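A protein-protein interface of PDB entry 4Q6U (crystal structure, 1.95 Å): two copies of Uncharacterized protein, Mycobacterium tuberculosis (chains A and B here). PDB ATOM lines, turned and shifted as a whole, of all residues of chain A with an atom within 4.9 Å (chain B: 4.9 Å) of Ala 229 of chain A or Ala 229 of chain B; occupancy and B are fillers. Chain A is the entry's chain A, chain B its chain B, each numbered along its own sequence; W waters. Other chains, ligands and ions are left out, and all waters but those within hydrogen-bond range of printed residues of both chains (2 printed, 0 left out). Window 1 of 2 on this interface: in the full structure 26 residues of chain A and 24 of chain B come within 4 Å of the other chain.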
ATOM      1  N   LEU A 153      14.453  -0.306 -33.269  1.00  0.00           N
ATOM      2  CA  LEU A 153      13.271  -0.849 -33.943  1.00  0.00           C
ATOM      3  C   LEU A 153      12.447   0.253 -34.603  1.00  0.00           C
ATOM      4  O   LEU A 153      12.438   1.395 -34.132  1.00  0.00           O
ATOM      5  CB  LEU A 153      12.390  -1.612 -32.943  1.00  0.00           C
ATOM      6  CG  LEU A 153      13.063  -2.763 -32.187  1.00  0.00           C
ATOM      7  CD1 LEU A 153      12.080  -3.448 -31.248  1.00  0.00           C
ATOM      8  CD2 LEU A 153      13.626  -3.746 -33.167  1.00  0.00           C
ATOM      9  N   ASP A 227       7.448   2.365 -25.717  1.00  0.00           N
ATOM     10  CA  ASP A 227       7.714   0.959 -26.003  1.00  0.00           C
ATOM     11  C   ASP A 227       8.308   0.250 -24.773  1.00  0.00           C
ATOM     12  O   ASP A 227       9.525   0.142 -24.618  1.00  0.00           O
ATOM     13  CB  ASP A 227       8.653   0.833 -27.218  1.00  0.00           C
ATOM     14  CG  ASP A 227       8.576  -0.540 -27.877  1.00  0.00           C
ATOM     15  OD1 ASP A 227       8.162  -1.501 -27.185  1.00  0.00           O
ATOM     16  OD2 ASP A 227       8.960  -0.666 -29.070  1.00  0.00           O
ATOM     17  N   LEU A 228       7.427  -0.214 -23.896  1.00  0.00           N
ATOM     18  CA  LEU A 228       7.830  -0.940 -22.701  1.00  0.00           C
ATOM     19  C   LEU A 228       8.569  -2.212 -23.088  1.00  0.00           C
ATOM     20  O   LEU A 228       9.615  -2.498 -22.532  1.00  0.00           O
ATOM     21  CB  LEU A 228       6.615  -1.278 -21.825  1.00  0.00           C
ATOM     22  CG  LEU A 228       6.877  -2.170 -20.599  1.00  0.00           C
ATOM     23  CD1 LEU A 228       7.950  -1.583 -19.695  1.00  0.00           C
ATOM     24  CD2 LEU A 228       5.595  -2.399 -19.793  1.00  0.00           C
ATOM     25  N   ALA A 229       8.028  -2.965 -24.043  1.00  0.00           N
ATOM     26  CA  ALA A 229       8.644  -4.234 -24.448  1.00  0.00           C
ATOM     27  C   ALA A 229      10.082  -4.052 -24.927  1.00  0.00           C
ATOM     28  O   ALA A 229      10.952  -4.884 -24.649  1.00  0.00           O
ATOM     29  CB  ALA A 229       7.802  -4.912 -25.533  1.00  0.00           C
ATOM     30  N   GLN A 230      10.341  -2.968 -25.649  1.00  0.00           N
ATOM     31  CA  GLN A 230      11.677  -2.656 -26.144  1.00  0.00           C
ATOM     32  C   GLN A 230      12.639  -2.456 -24.982  1.00  0.00           C
ATOM     33  O   GLN A 230      13.775  -2.919 -25.000  1.00  0.00           O
ATOM     34  CB  GLN A 230      11.627  -1.403 -27.024  1.00  0.00           C
ATOM     35  CG  GLN A 230      12.886  -1.118 -27.820  1.00  0.00           C
ATOM     36  CD  GLN A 230      12.684  -0.030 -28.872  1.00  0.00           C
ATOM     37  OE1 GLN A 230      11.557   0.394 -29.156  1.00  0.00           O
ATOM     38  NE2 GLN A 230      13.783   0.426 -29.448  1.00  0.00           N
ATOM     39  N   ARG A 231      12.163  -1.754 -23.958  1.00  0.00           N
ATOM     40  CA  ARG A 231      13.000  -1.509 -22.795  1.00  0.00           C
ATOM     41  C   ARG A 231      13.330  -2.816 -22.078  1.00  0.00           C
ATOM     42  O   ARG A 231      14.434  -2.979 -21.563  1.00  0.00           O
ATOM     43  CB  ARG A 231      12.315  -0.526 -21.836  1.00  0.00           C
ATOM     44  CG  ARG A 231      12.263   0.878 -22.418  1.00  0.00           C
ATOM     45  CD  ARG A 231      11.454   1.839 -21.577  1.00  0.00           C
ATOM     46  NE  ARG A 231      11.489   3.176 -22.164  1.00  0.00           N
ATOM     47  CZ  ARG A 231      12.456   4.060 -21.945  1.00  0.00           C
ATOM     48  NH1 ARG A 231      13.463   3.757 -21.136  1.00  0.00           N
ATOM     49  NH2 ARG A 231      12.413   5.251 -22.526  1.00  0.00           N
ATOM     50  N   ILE A 232      12.362  -3.729 -22.026  1.00  0.00           N
ATOM     51  CA  ILE A 232      12.574  -5.022 -21.386  1.00  0.00           C
ATOM     52  C   ILE A 232      13.558  -5.842 -22.220  1.00  0.00           C
ATOM     53  O   ILE A 232      14.471  -6.483 -21.697  1.00  0.00           O
ATOM     54  CB  ILE A 232      11.256  -5.783 -21.224  1.00  0.00           C
ATOM     55  CG1 ILE A 232      10.341  -5.040 -20.233  1.00  0.00           C
ATOM     56  CG2 ILE A 232      11.502  -7.204 -20.740  1.00  0.00           C
ATOM     57  CD1 ILE A 232       8.899  -5.491 -20.292  1.00  0.00           C
ATOM     58  N   LEU A 233      13.377  -5.783 -23.529  1.00  0.00           N
ATOM     59  CA  LEU A 233      14.236  -6.521 -24.443  1.00  0.00           C
ATOM     60  C   LEU A 233      15.679  -6.051 -24.298  1.00  0.00           C
ATOM     61  O   LEU A 233      16.613  -6.853 -24.312  1.00  0.00           O
ATOM     62  CB  LEU A 233      13.744  -6.344 -25.882  1.00  0.00           C
ATOM     63  CG  LEU A 233      13.909  -7.502 -26.861  1.00  0.00           C
ATOM     64  CD1 LEU A 233      13.373  -8.805 -26.264  1.00  0.00           C
ATOM     65  CD2 LEU A 233      13.186  -7.146 -28.164  1.00  0.00           C
ATOM     66  N   LEU B 153       0.249  -5.234 -23.005  1.00  0.00           N
ATOM     67  CA  LEU B 153       0.840  -3.931 -22.716  1.00  0.00           C
ATOM     68  C   LEU B 153      -0.053  -2.794 -23.213  1.00  0.00           C
ATOM     69  O   LEU B 153      -0.757  -2.942 -24.205  1.00  0.00           O
ATOM     70  CB  LEU B 153       2.225  -3.819 -23.373  1.00  0.00           C
ATOM     71  CG  LEU B 153       3.204  -4.950 -23.038  1.00  0.00           C
ATOM     72  CD1 LEU B 153       4.533  -4.694 -23.753  1.00  0.00           C
ATOM     73  CD2 LEU B 153       3.411  -5.061 -21.558  1.00  0.00           C
ATOM     74  N   ASP B 227       4.153  -3.943 -32.986  1.00  0.00           N
ATOM     75  CA  ASP B 227       5.002  -4.070 -31.803  1.00  0.00           C
ATOM     76  C   ASP B 227       5.891  -5.309 -31.916  1.00  0.00           C
ATOM     77  O   ASP B 227       5.580  -6.367 -31.373  1.00  0.00           O
ATOM     78  CB  ASP B 227       4.147  -4.144 -30.529  1.00  0.00           C
ATOM     79  CG  ASP B 227       4.947  -3.854 -29.260  1.00  0.00           C
ATOM     80  OD1 ASP B 227       6.198  -3.929 -29.311  1.00  0.00           O
ATOM     81  OD2 ASP B 227       4.322  -3.568 -28.201  1.00  0.00           O
ATOM     82  N   LEU B 228       6.991  -5.160 -32.643  1.00  0.00           N
ATOM     83  CA  LEU B 228       7.948  -6.246 -32.860  1.00  0.00           C
ATOM     84  C   LEU B 228       8.562  -6.694 -31.525  1.00  0.00           C
ATOM     85  O   LEU B 228       8.714  -7.891 -31.272  1.00  0.00           O
ATOM     86  CB  LEU B 228       9.031  -5.778 -33.843  1.00  0.00           C
ATOM     87  CG  LEU B 228      10.231  -6.671 -34.192  1.00  0.00           C
ATOM     88  CD1 LEU B 228       9.783  -8.014 -34.745  1.00  0.00           C
ATOM     89  CD2 LEU B 228      11.071  -5.938 -35.227  1.00  0.00           C
ATOM     90  N   ALA B 229       8.897  -5.738 -30.664  1.00  0.00           N
ATOM     91  CA  ALA B 229       9.515  -6.088 -29.383  1.00  0.00           C
ATOM     92  C   ALA B 229       8.591  -6.978 -28.547  1.00  0.00           C
ATOM     93  O   ALA B 229       9.028  -7.944 -27.908  1.00  0.00           O
ATOM     94  CB  ALA B 229       9.893  -4.836 -28.611  1.00  0.00           C
ATOM     95  N   GLN B 230       7.300  -6.659 -28.552  1.00  0.00           N
ATOM     96  CA  GLN B 230       6.347  -7.465 -27.794  1.00  0.00           C
ATOM     97  C   GLN B 230       6.247  -8.877 -28.380  1.00  0.00           C
ATOM     98  O   GLN B 230       6.122  -9.840 -27.638  1.00  0.00           O
ATOM     99  CB  GLN B 230       4.965  -6.789 -27.743  1.00  0.00           C
ATOM    100  CG  GLN B 230       3.826  -7.654 -27.148  1.00  0.00           C
ATOM    101  CD  GLN B 230       3.937  -7.898 -25.634  1.00  0.00           C
ATOM    102  OE1 GLN B 230       5.014  -7.790 -25.043  1.00  0.00           O
ATOM    103  NE2 GLN B 230       2.806  -8.237 -25.007  1.00  0.00           N
ATOM    104  N   ARG B 231       6.336  -9.008 -29.701  1.00  0.00           N
ATOM    105  CA  ARG B 231       6.275 -10.333 -30.302  1.00  0.00           C
ATOM    106  C   ARG B 231       7.521 -11.155 -29.926  1.00  0.00           C
ATOM    107  O   ARG B 231       7.436 -12.351 -29.665  1.00  0.00           O
ATOM    108  CB  ARG B 231       6.123 -10.214 -31.817  1.00  0.00           C
ATOM    109  CG  ARG B 231       4.752  -9.681 -32.237  1.00  0.00           C
ATOM    110  CD  ARG B 231       4.671  -9.393 -33.734  1.00  0.00           C
ATOM    111  NE  ARG B 231       3.309  -9.050 -34.140  1.00  0.00           N
ATOM    112  CZ  ARG B 231       2.355  -9.944 -34.390  1.00  0.00           C
ATOM    113  NH1 ARG B 231       2.609 -11.243 -34.283  1.00  0.00           N
ATOM    114  NH2 ARG B 231       1.145  -9.541 -34.747  1.00  0.00           N
ATOM    115  N   ILE B 232       8.666 -10.491 -29.876  1.00  0.00           N
ATOM    116  CA  ILE B 232       9.905 -11.123 -29.438  1.00  0.00           C
ATOM    117  C   ILE B 232       9.789 -11.522 -27.947  1.00  0.00           C
ATOM    118  O   ILE B 232      10.115 -12.640 -27.563  1.00  0.00           O
ATOM    119  CB  ILE B 232      11.106 -10.174 -29.684  1.00  0.00           C
ATOM    120  CG1 ILE B 232      11.295  -9.949 -31.209  1.00  0.00           C
ATOM    121  CG2 ILE B 232      12.388 -10.744 -29.095  1.00  0.00           C
ATOM    122  CD1 ILE B 232      12.318  -8.898 -31.533  1.00  0.00           C
ATOM    123  N   LEU B 233       9.278 -10.615 -27.127  1.00  0.00           N
ATOM    124  CA  LEU B 233       9.155 -10.888 -25.695  1.00  0.00           C
ATOM    125  C   LEU B 233       8.254 -12.096 -25.437  1.00  0.00           C
ATOM    126  O   LEU B 233       8.569 -12.971 -24.616  1.00  0.00           O
ATOM    127  CB  LEU B 233       8.612  -9.640 -24.982  1.00  0.00           C
ATOM    128  CG  LEU B 233       9.245  -9.213 -23.668  1.00  0.00           C
ATOM    129  CD1 LEU B 233      10.747  -9.034 -23.845  1.00  0.00           C
ATOM    130  CD2 LEU B 233       8.606  -7.915 -23.217  1.00  0.00           C
HETATM  131  O   HOH W   1       8.082  -2.653 -30.484  1.00  0.00           O
HETATM  132  O   HOH W   2       5.926  -2.149 -26.323  1.00  0.00           O
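The side-chain amide oxygen of Gln 230 of chain A sits close to the side-chain carboxylate of Asp 227 of chain A (2.8 Å).
The backbone NH (N) of Gln 230 of chain B sits at hydrogen-bond distance from the side-chain carboxylate (OD1) of Asp 227 of chain B (3.0 Å).
OD1 of Asp 227 of chain A lies close to N of Ala 229 of chain A (3.5 Å).
Leu 153 of chain A touches Leu 228 of chain B.
Ala 229 of chain B touches Leu 153 of chain A.
CD2 of Leu 153 of chain B touches CD2 of Leu 228 of chain A (3.9 Å).
Leu 153 of chain B touches Ala 229 of chain A.
CB of Ala 229 of chain A touches CB of Ala 229 of chain B, at 3.7 Å.
N of Gln 230 of chain B touches CB of Ala 229 of chain A, 3.5 Å away.
Ala 229 of chain A touches Leu 233 of chain B (CB to CD2, 3.9 Å).
Leu 233 of chain B touches Ile 232 of chain A (CD1 to CG2, 3.7 Å).
Leu 233 of chain A touches Ile 232 of chain B.
Leu 233 of chain A touches Leu 233 of chain B (CD1 to CD1, 3.6 Å).
Of the printed residues of chain B, Leu 153 of chain A touches Leu 228 (3.9 Å) and Ala 229 (3.7 Å).
Of the printed residues of chain B, Asp 227 of chain A touches Asp 227.
Ala 229 of chain A touches just these residues of chain B: Leu 153, Ala 229, Gln 230 and Leu 233.
Arg 231 of chain A touches none of the printed residues of chain B.
Printed residues of chain B within 4 Å of Leu 233 of chain A: Ile 232 and Leu 233.
Of the printed residues of chain A, Ala 229 of chain B touches Leu 153, Ala 229 and Gln 230.
Arg 231 of chain B touches none of the printed residues of chain A.
Of the printed residues of chain A, Ile 232 of chain B touches Leu 233 (3.6 Å).
The nearest residue of chain B that does not touch Ala 229 of chain A is Asp 227 of chain B (4.2 Å).
Of the 8 printed residues of chain B, 7 touch a printed residue of chain A.
Of the 8 printed residues of chain A, 7 touch a printed residue of chain B.
Among the printed residues, no Asp or Glu carboxylate lies within 4 Å of a Lys or Arg side-chain nitrogen of the other chain.
Leu 153 of chain A touches Leu 228 of chain B, and with the chains exchanged Leu 228 of chain A touches Leu 153 of chain B.
Leu 153 of chain A touches Ala 229 of chain B, and with the chains exchanged Ala 229 of chain A touches Leu 153 of chain B.
Ala 229 of chain A touches Gln 230 of chain B, and with the chains exchanged Gln 230 of chain A touches Ala 229 of chain B.
Leu 233 of chain A touches its own counterpart, Leu 233 of chain B.
8 positions are printed for both chains.
Water W2 lies within hydrogen-bond range of OD1 of Asp 227 of chain A (2.5 Å), OD2 of Asp 227 of chain B (2.8 Å), N of Ala 229 of chain A (3.2 Å) and N of Leu 228 of chain A (3.4 Å).
Water W1 lies within hydrogen-bond range of the side-chain carboxylate (OD1) of Asp 227 of chain B (2.6 Å), the side-chain carboxylate (OD2) of Asp 227 of chain A (2.6 Å), the backbone NH (N) of Ala 229 of chain B (3.2 Å) and the backbone NH (N) of Leu 228 of chain B (3.5 Å).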
